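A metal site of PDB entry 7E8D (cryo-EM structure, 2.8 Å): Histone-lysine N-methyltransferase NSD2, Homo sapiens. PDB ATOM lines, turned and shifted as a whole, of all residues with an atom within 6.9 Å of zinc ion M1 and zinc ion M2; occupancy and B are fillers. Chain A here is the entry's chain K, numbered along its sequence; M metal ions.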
ATOM      1  N   LYS A  43     -18.275  -9.221  -8.743  1.00  0.00           N
ATOM      2  CA  LYS A  43     -18.613  -9.513 -10.118  1.00  0.00           C
ATOM      3  C   LYS A  43     -20.108  -9.730 -10.219  1.00  0.00           C
ATOM      4  O   LYS A  43     -20.681 -10.466  -9.403  1.00  0.00           O
ATOM      5  CB  LYS A  43     -17.856 -10.752 -10.600  1.00  0.00           C
ATOM      6  CG  LYS A  43     -18.116 -11.116 -12.041  1.00  0.00           C
ATOM      7  CD  LYS A  43     -18.434 -12.598 -12.190  1.00  0.00           C
ATOM      8  CE  LYS A  43     -17.328 -13.444 -11.594  1.00  0.00           C
ATOM      9  NZ  LYS A  43     -17.713 -14.879 -11.626  1.00  0.00           N
ATOM     10  N   CYS A  44     -20.738  -9.111 -11.201  1.00  0.00           N
ATOM     11  CA  CYS A  44     -22.191  -9.177 -11.320  1.00  0.00           C
ATOM     12  C   CYS A  44     -22.601 -10.433 -12.085  1.00  0.00           C
ATOM     13  O   CYS A  44     -21.806 -11.345 -12.317  1.00  0.00           O
ATOM     14  CB  CYS A  44     -22.722  -7.919 -11.991  1.00  0.00           C
ATOM     15  SG  CYS A  44     -22.102  -7.634 -13.640  1.00  0.00           S
ATOM     16  N   ASN A  45     -23.874 -10.483 -12.476  1.00  0.00           N
ATOM     17  CA  ASN A  45     -24.416 -11.576 -13.271  1.00  0.00           C
ATOM     18  C   ASN A  45     -24.837 -11.121 -14.653  1.00  0.00           C
ATOM     19  O   ASN A  45     -25.486 -11.874 -15.369  1.00  0.00           O
ATOM     20  CB  ASN A  45     -25.598 -12.215 -12.553  1.00  0.00           C
ATOM     21  CG  ASN A  45     -25.180 -12.999 -11.331  1.00  0.00           C
ATOM     22  OD1 ASN A  45     -24.153 -13.656 -11.338  1.00  0.00           O
ATOM     23  ND2 ASN A  45     -25.983 -12.920 -10.286  1.00  0.00           N
ATOM     24  N   CYS A  46     -24.482  -9.893 -15.039  1.00  0.00           N
ATOM     25  CA  CYS A  46     -24.849  -9.405 -16.353  1.00  0.00           C
ATOM     26  C   CYS A  46     -24.087 -10.180 -17.425  1.00  0.00           C
ATOM     27  O   CYS A  46     -23.003 -10.717 -17.198  1.00  0.00           O
ATOM     28  CB  CYS A  46     -24.551  -7.914 -16.465  1.00  0.00           C
ATOM     29  SG  CYS A  46     -25.504  -6.894 -15.328  1.00  0.00           S
ATOM     30  N   LYS A  47     -24.692 -10.246 -18.615  1.00  0.00           N
ATOM     31  CA  LYS A  47     -24.095 -11.005 -19.688  1.00  0.00           C
ATOM     32  C   LYS A  47     -23.758 -10.100 -20.866  1.00  0.00           C
ATOM     33  O   LYS A  47     -24.468  -9.124 -21.118  1.00  0.00           O
ATOM     34  CB  LYS A  47     -25.035 -12.122 -20.152  1.00  0.00           C
ATOM     35  CG  LYS A  47     -25.322 -13.145 -19.077  1.00  0.00           C
ATOM     36  CD  LYS A  47     -26.295 -14.201 -19.575  1.00  0.00           C
ATOM     37  CE  LYS A  47     -27.625 -13.579 -19.938  1.00  0.00           C
ATOM     38  NZ  LYS A  47     -28.177 -12.851 -18.782  1.00  0.00           N
ATOM     39  N   ASP A  50     -26.538  -9.060 -23.312  1.00  0.00           N
ATOM     40  CA  ASP A  50     -27.736  -8.432 -22.803  1.00  0.00           C
ATOM     41  C   ASP A  50     -28.058  -7.172 -23.593  1.00  0.00           C
ATOM     42  O   ASP A  50     -27.285  -6.706 -24.432  1.00  0.00           O
ATOM     43  CB  ASP A  50     -27.576  -8.112 -21.319  1.00  0.00           C
ATOM     44  CG  ASP A  50     -27.324  -9.351 -20.480  1.00  0.00           C
ATOM     45  OD1 ASP A  50     -27.699 -10.448 -20.934  1.00  0.00           O
ATOM     46  OD2 ASP A  50     -26.752  -9.228 -19.374  1.00  0.00           O
ATOM     47  N   ASN A  52     -28.369  -4.097 -22.473  1.00  0.00           N
ATOM     48  CA  ASN A  52     -27.408  -3.073 -22.073  1.00  0.00           C
ATOM     49  C   ASN A  52     -26.631  -3.616 -20.895  1.00  0.00           C
ATOM     50  O   ASN A  52     -26.982  -3.370 -19.739  1.00  0.00           O
ATOM     51  CB  ASN A  52     -28.077  -1.757 -21.716  1.00  0.00           C
ATOM     52  CG  ASN A  52     -28.231  -0.845 -22.905  1.00  0.00           C
ATOM     53  OD1 ASN A  52     -27.253  -0.341 -23.445  1.00  0.00           O
ATOM     54  ND2 ASN A  52     -29.465  -0.618 -23.323  1.00  0.00           N
ATOM     55  N   PRO A  53     -25.548  -4.354 -21.147  1.00  0.00           N
ATOM     56  CA  PRO A  53     -24.851  -5.037 -20.061  1.00  0.00           C
ATOM     57  C   PRO A  53     -24.339  -4.057 -19.028  1.00  0.00           C
ATOM     58  O   PRO A  53     -23.593  -3.123 -19.345  1.00  0.00           O
ATOM     59  CB  PRO A  53     -23.692  -5.746 -20.785  1.00  0.00           C
ATOM     60  CG  PRO A  53     -24.125  -5.829 -22.194  1.00  0.00           C
ATOM     61  CD  PRO A  53     -24.925  -4.598 -22.453  1.00  0.00           C
ATOM     62  N   CYS A  54     -24.751  -4.263 -17.784  1.00  0.00           N
ATOM     63  CA  CYS A  54     -24.392  -3.386 -16.676  1.00  0.00           C
ATOM     64  C   CYS A  54     -24.820  -1.950 -16.946  1.00  0.00           C
ATOM     65  O   CYS A  54     -24.208  -1.012 -16.462  1.00  0.00           O
ATOM     66  CB  CYS A  54     -22.905  -3.468 -16.386  1.00  0.00           C
ATOM     67  SG  CYS A  54     -22.302  -5.140 -16.281  1.00  0.00           S
ATOM     68  N   GLY A  55     -25.878  -1.790 -17.730  1.00  0.00           N
ATOM     69  CA  GLY A  55     -26.328  -0.474 -18.104  1.00  0.00           C
ATOM     70  C   GLY A  55     -26.960   0.268 -16.949  1.00  0.00           C
ATOM     71  O   GLY A  55     -27.173  -0.271 -15.864  1.00  0.00           O
ATOM     72  N   SER A  58     -30.556  -1.166 -16.278  1.00  0.00           N
ATOM     73  CA  SER A  58     -30.660  -2.607 -16.139  1.00  0.00           C
ATOM     74  C   SER A  58     -30.623  -2.990 -14.662  1.00  0.00           C
ATOM     75  O   SER A  58     -30.672  -2.143 -13.773  1.00  0.00           O
ATOM     76  CB  SER A  58     -29.546  -3.283 -16.935  1.00  0.00           C
ATOM     77  OG  SER A  58     -28.288  -2.711 -16.617  1.00  0.00           O
ATOM     78  N   GLU A  59     -30.540  -4.293 -14.390  1.00  0.00           N
ATOM     79  CA  GLU A  59     -30.492  -4.806 -13.026  1.00  0.00           C
ATOM     80  C   GLU A  59     -29.087  -5.218 -12.616  1.00  0.00           C
ATOM     81  O   GLU A  59     -28.914  -6.241 -11.951  1.00  0.00           O
ATOM     82  CB  GLU A  59     -31.451  -5.986 -12.865  1.00  0.00           C
ATOM     83  CG  GLU A  59     -32.897  -5.601 -12.622  1.00  0.00           C
ATOM     84  CD  GLU A  59     -33.542  -5.014 -13.852  1.00  0.00           C
ATOM     85  OE1 GLU A  59     -33.061  -5.297 -14.966  1.00  0.00           O
ATOM     86  OE2 GLU A  59     -34.527  -4.259 -13.701  1.00  0.00           O
ATOM     87  N   CYS A  60     -28.069  -4.457 -13.011  1.00  0.00           N
ATOM     88  CA  CYS A  60     -26.703  -4.822 -12.655  1.00  0.00           C
ATOM     89  C   CYS A  60     -26.549  -4.875 -11.148  1.00  0.00           C
ATOM     90  O   CYS A  60     -26.880  -3.928 -10.446  1.00  0.00           O
ATOM     91  CB  CYS A  60     -25.714  -3.840 -13.254  1.00  0.00           C
ATOM     92  SG  CYS A  60     -23.995  -4.310 -12.990  1.00  0.00           S
ATOM     93  N   LEU A  61     -26.030  -5.989 -10.667  1.00  0.00           N
ATOM     94  CA  LEU A  61     -25.864  -6.169  -9.232  1.00  0.00           C
ATOM     95  C   LEU A  61     -24.713  -5.344  -8.679  1.00  0.00           C
ATOM     96  O   LEU A  61     -24.642  -5.147  -7.469  1.00  0.00           O
ATOM     97  CB  LEU A  61     -25.635  -7.642  -8.930  1.00  0.00           C
ATOM     98  CG  LEU A  61     -26.008  -8.101  -7.530  1.00  0.00           C
ATOM     99  CD1 LEU A  61     -27.305  -7.471  -7.111  1.00  0.00           C
ATOM    100  CD2 LEU A  61     -26.130  -9.589  -7.528  1.00  0.00           C
ATOM    101  N   ASN A  62     -23.816  -4.867  -9.528  1.00  0.00           N
ATOM    102  CA  ASN A  62     -22.799  -3.936  -9.063  1.00  0.00           C
ATOM    103  C   ASN A  62     -23.331  -2.519  -9.062  1.00  0.00           C
ATOM    104  O   ASN A  62     -23.021  -1.726  -8.159  1.00  0.00           O
ATOM    105  CB  ASN A  62     -21.553  -4.027  -9.926  1.00  0.00           C
ATOM    106  CG  ASN A  62     -20.703  -5.214  -9.589  1.00  0.00           C
ATOM    107  OD1 ASN A  62     -21.056  -6.336  -9.891  1.00  0.00           O
ATOM    108  ND2 ASN A  62     -19.567  -4.974  -8.960  1.00  0.00           N
ATOM    109  N   ARG A  63     -24.120  -2.172 -10.077  1.00  0.00           N
ATOM    110  CA  ARG A  63     -24.682  -0.823 -10.133  1.00  0.00           C
ATOM    111  C   ARG A  63     -25.681  -0.607  -9.016  1.00  0.00           C
ATOM    112  O   ARG A  63     -25.729   0.465  -8.422  1.00  0.00           O
ATOM    113  CB  ARG A  63     -25.320  -0.593 -11.501  1.00  0.00           C
ATOM    114  CG  ARG A  63     -25.555   0.867 -11.793  1.00  0.00           C
ATOM    115  CD  ARG A  63     -26.205   1.073 -13.130  1.00  0.00           C
ATOM    116  NE  ARG A  63     -25.284   0.926 -14.241  1.00  0.00           N
ATOM    117  CZ  ARG A  63     -24.590   1.935 -14.772  1.00  0.00           C
ATOM    118  NH1 ARG A  63     -24.723   3.152 -14.277  1.00  0.00           N
ATOM    119  NH2 ARG A  63     -23.778   1.712 -15.788  1.00  0.00           N
ATOM    120  N   GLU A  68     -18.478  -0.479  -8.846  1.00  0.00           N
ATOM    121  CA  GLU A  68     -18.045  -0.220 -10.203  1.00  0.00           C
ATOM    122  C   GLU A  68     -17.505  -1.511 -10.793  1.00  0.00           C
ATOM    123  O   GLU A  68     -16.640  -2.156 -10.200  1.00  0.00           O
ATOM    124  CB  GLU A  68     -16.976   0.870 -10.218  1.00  0.00           C
ATOM    125  CG  GLU A  68     -16.420   1.172 -11.578  1.00  0.00           C
ATOM    126  CD  GLU A  68     -17.151   2.305 -12.262  1.00  0.00           C
ATOM    127  OE1 GLU A  68     -18.366   2.451 -12.053  1.00  0.00           O
ATOM    128  OE2 GLU A  68     -16.497   3.053 -13.008  1.00  0.00           O
ATOM    129  N   CYS A  69     -18.018  -1.894 -11.963  1.00  0.00           N
ATOM    130  CA  CYS A  69     -17.521  -3.098 -12.608  1.00  0.00           C
ATOM    131  C   CYS A  69     -16.079  -2.881 -13.059  1.00  0.00           C
ATOM    132  O   CYS A  69     -15.599  -1.750 -13.158  1.00  0.00           O
ATOM    133  CB  CYS A  69     -18.398  -3.473 -13.799  1.00  0.00           C
ATOM    134  SG  CYS A  69     -19.888  -4.367 -13.377  1.00  0.00           S
ATOM    135  N   HIS A  70     -15.397  -3.984 -13.309  1.00  0.00           N
ATOM    136  CA  HIS A  70     -14.021  -3.972 -13.767  1.00  0.00           C
ATOM    137  C   HIS A  70     -13.964  -4.746 -15.072  1.00  0.00           C
ATOM    138  O   HIS A  70     -14.440  -5.896 -15.132  1.00  0.00           O
ATOM    139  CB  HIS A  70     -13.100  -4.600 -12.724  1.00  0.00           C
ATOM    140  CG  HIS A  70     -11.648  -4.433 -13.011  1.00  0.00           C
ATOM    141  ND1 HIS A  70     -11.070  -4.845 -14.196  1.00  0.00           N
ATOM    142  CD2 HIS A  70     -10.646  -3.925 -12.269  1.00  0.00           C
ATOM    143  CE1 HIS A  70      -9.781  -4.588 -14.159  1.00  0.00           C
ATOM    144  NE2 HIS A  70      -9.492  -4.020 -13.001  1.00  0.00           N
ATOM    145  N   PRO A  71     -13.417  -4.162 -16.139  1.00  0.00           N
ATOM    146  CA  PRO A  71     -13.469  -4.837 -17.449  1.00  0.00           C
ATOM    147  C   PRO A  71     -12.771  -6.184 -17.454  1.00  0.00           C
ATOM    148  O   PRO A  71     -13.171  -7.076 -18.221  1.00  0.00           O
ATOM    149  CB  PRO A  71     -12.780  -3.834 -18.382  1.00  0.00           C
ATOM    150  CG  PRO A  71     -11.882  -3.054 -17.476  1.00  0.00           C
ATOM    151  CD  PRO A  71     -12.614  -2.924 -16.183  1.00  0.00           C
ATOM    152  N   CYS A  74     -15.590  -8.068 -14.980  1.00  0.00           N
ATOM    153  CA  CYS A  74     -16.980  -8.086 -15.373  1.00  0.00           C
ATOM    154  C   CYS A  74     -17.194  -9.134 -16.460  1.00  0.00           C
ATOM    155  O   CYS A  74     -16.452  -9.156 -17.449  1.00  0.00           O
ATOM    156  CB  CYS A  74     -17.419  -6.721 -15.869  1.00  0.00           C
ATOM    157  SG  CYS A  74     -19.137  -6.626 -16.331  1.00  0.00           S
ATOM    158  N   PRO A  75     -18.184 -10.017 -16.318  1.00  0.00           N
ATOM    159  CA  PRO A  75     -18.443 -10.994 -17.380  1.00  0.00           C
ATOM    160  C   PRO A  75     -18.886 -10.383 -18.681  1.00  0.00           C
ATOM    161  O   PRO A  75     -18.799 -11.044 -19.712  1.00  0.00           O
ATOM    162  CB  PRO A  75     -19.541 -11.876 -16.767  1.00  0.00           C
ATOM    163  CG  PRO A  75     -20.216 -10.992 -15.802  1.00  0.00           C
ATOM    164  CD  PRO A  75     -19.151 -10.131 -15.221  1.00  0.00           C
ATOM    165  N   ALA A  76     -19.376  -9.142 -18.670  1.00  0.00           N
ATOM    166  CA  ALA A  76     -19.756  -8.494 -19.903  1.00  0.00           C
ATOM    167  C   ALA A  76     -18.559  -8.025 -20.711  1.00  0.00           C
ATOM    168  O   ALA A  76     -18.736  -7.553 -21.833  1.00  0.00           O
ATOM    169  CB  ALA A  76     -20.670  -7.301 -19.619  1.00  0.00           C
ATOM    170  N   GLY A  77     -17.352  -8.137 -20.160  1.00  0.00           N
ATOM    171  CA  GLY A  77     -16.156  -7.781 -20.890  1.00  0.00           C
ATOM    172  C   GLY A  77     -16.059  -6.298 -21.182  1.00  0.00           C
ATOM    173  O   GLY A  77     -15.803  -5.502 -20.279  1.00  0.00           O
ATOM    174  N   PHE A  79     -18.637  -4.746 -23.039  1.00  0.00           N
ATOM    175  CA  PHE A  79     -19.990  -4.224 -23.175  1.00  0.00           C
ATOM    176  C   PHE A  79     -20.522  -3.639 -21.870  1.00  0.00           C
ATOM    177  O   PHE A  79     -21.720  -3.336 -21.792  1.00  0.00           O
ATOM    178  CB  PHE A  79     -20.925  -5.330 -23.670  1.00  0.00           C
ATOM    179  CG  PHE A  79     -20.523  -5.909 -24.985  1.00  0.00           C
ATOM    180  CD1 PHE A  79     -19.591  -6.933 -25.060  1.00  0.00           C
ATOM    181  CD2 PHE A  79     -21.074  -5.434 -26.158  1.00  0.00           C
ATOM    182  CE1 PHE A  79     -19.235  -7.468 -26.278  1.00  0.00           C
ATOM    183  CE2 PHE A  79     -20.718  -5.969 -27.377  1.00  0.00           C
ATOM    184  CZ  PHE A  79     -19.789  -6.982 -27.432  1.00  0.00           C
ATOM    185  N   CYS A  80     -19.666  -3.485 -20.865  1.00  0.00           N
ATOM    186  CA  CYS A  80     -20.081  -3.018 -19.553  1.00  0.00           C
ATOM    187  C   CYS A  80     -20.172  -1.500 -19.567  1.00  0.00           C
ATOM    188  O   CYS A  80     -19.143  -0.811 -19.648  1.00  0.00           O
ATOM    189  CB  CYS A  80     -19.087  -3.492 -18.499  1.00  0.00           C
ATOM    190  SG  CYS A  80     -19.333  -2.795 -16.850  1.00  0.00           S
ATOM    191  N   GLN A  81     -21.386  -0.967 -19.473  1.00  0.00           N
ATOM    192  CA  GLN A  81     -21.593   0.467 -19.333  1.00  0.00           C
ATOM    193  C   GLN A  81     -21.493   0.923 -17.888  1.00  0.00           C
ATOM    194  O   GLN A  81     -22.047   1.970 -17.543  1.00  0.00           O
ATOM    195  CB  GLN A  81     -22.947   0.875 -19.912  1.00  0.00           C
ATOM    196  CG  GLN A  81     -23.119   0.562 -21.386  1.00  0.00           C
ATOM    197  CD  GLN A  81     -23.778  -0.769 -21.606  1.00  0.00           C
ATOM    198  OE1 GLN A  81     -24.709  -1.129 -20.894  1.00  0.00           O
ATOM    199  NE2 GLN A  81     -23.292  -1.510 -22.601  1.00  0.00           N
ATOM    200  N   ASN A  82     -20.835   0.157 -17.047  1.00  0.00           N
ATOM    201  CA  ASN A  82     -20.665   0.476 -15.634  1.00  0.00           C
ATOM    202  C   ASN A  82     -19.199   0.698 -15.293  1.00  0.00           C
ATOM    203  O   ASN A  82     -18.685   0.199 -14.289  1.00  0.00           O
ATOM    204  CB  ASN A  82     -21.276  -0.631 -14.765  1.00  0.00           C
ATOM    205  CG  ASN A  82     -21.236  -0.301 -13.292  1.00  0.00           C
ATOM    206  OD1 ASN A  82     -21.030   0.848 -12.902  1.00  0.00           O
ATOM    207  ND2 ASN A  82     -21.403  -1.317 -12.458  1.00  0.00           N
ATOM    208  N   GLN A  83     -18.490   1.438 -16.129  1.00  0.00           N
ATOM    209  CA  GLN A  83     -17.128   1.833 -15.839  1.00  0.00           C
ATOM    210  C   GLN A  83     -16.994   3.345 -15.873  1.00  0.00           C
ATOM    211  O   GLN A  83     -15.963   3.886 -16.274  1.00  0.00           O
ATOM    212  CB  GLN A  83     -16.147   1.163 -16.797  1.00  0.00           C
ATOM    213  CG  GLN A  83     -16.167  -0.336 -16.694  1.00  0.00           C
ATOM    214  CD  GLN A  83     -15.395  -0.993 -17.803  1.00  0.00           C
ATOM    215  OE1 GLN A  83     -14.207  -0.732 -17.977  1.00  0.00           O
ATOM    216  NE2 GLN A  83     -16.061  -1.850 -18.553  1.00  0.00           N
HETATM  217 ZN    ZN M   1     -20.133  -4.641 -15.665  1.00  0.00          ZN
HETATM  218 ZN    ZN M   2     -23.519  -6.011 -14.506  1.00  0.00          ZN
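SG of Cys 44 is bound to zinc ion M2 (2.3 Å).
SG of Cys 54 is bound to zinc ion M2 (2.3 Å).
SG of Cys 46 binds zinc ion M2, 2.3 Å away.
Zinc ion M2 is bound by SG of Cys 60.
The backbone carbonyl oxygen (O) of Cys 54 sits at hydrogen-bond distance from the guanidinium group (NH2) of Arg 63, 2.8 Å away.
The backbone NH (N) of Cys 69 is in hydrogen-bond range of the backbone carbonyl oxygen (O) of Asn 82, 3.2 Å away.
The side-chain sulfur (SG) of Cys 74 lies close to the backbone NH (N) of Ala 76 (3.4 Å).
The backbone NH of Cys 44 is in hydrogen-bond range of the side-chain amide oxygen of Asn 62, 3.1 Å away.
The side-chain sulfur of Cys 60 lies close to the backbone NH of Asn 62 (3.5 Å).
The side-chain sulfur (SG) of Cys 60 lies close to the backbone NH (N) of Arg 63.
The side-chain sulfur (SG) of Cys 80 sits close to the backbone NH (N) of Asn 82 (3.3 Å).
The backbone carbonyl oxygen (O) of Cys 80 is in hydrogen-bond range of the side-chain amide nitrogen (NE2) of Gln 83 (3.4 Å).
Along chain A the residues within 4 Å of zinc ion M2 span positions 44 to 60.
Zinc ion M1 is bound by the side-chain sulfur of Cys 54 (2.3 Å), the side-chain sulfur of Cys 69 (2.3 Å), the side-chain sulfur of Cys 74 (2.3 Å) and the side-chain sulfur of Cys 80 (2.3 Å).
Zinc ion M1 has four donor atoms within binding distance.
Within 4 Å of zinc ion M1: Cys 54, Cys 69, Cys 74 and Cys 80.
The nearest printed residue that does not touch zinc ion M1 is Cys 44 (4.1 Å).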
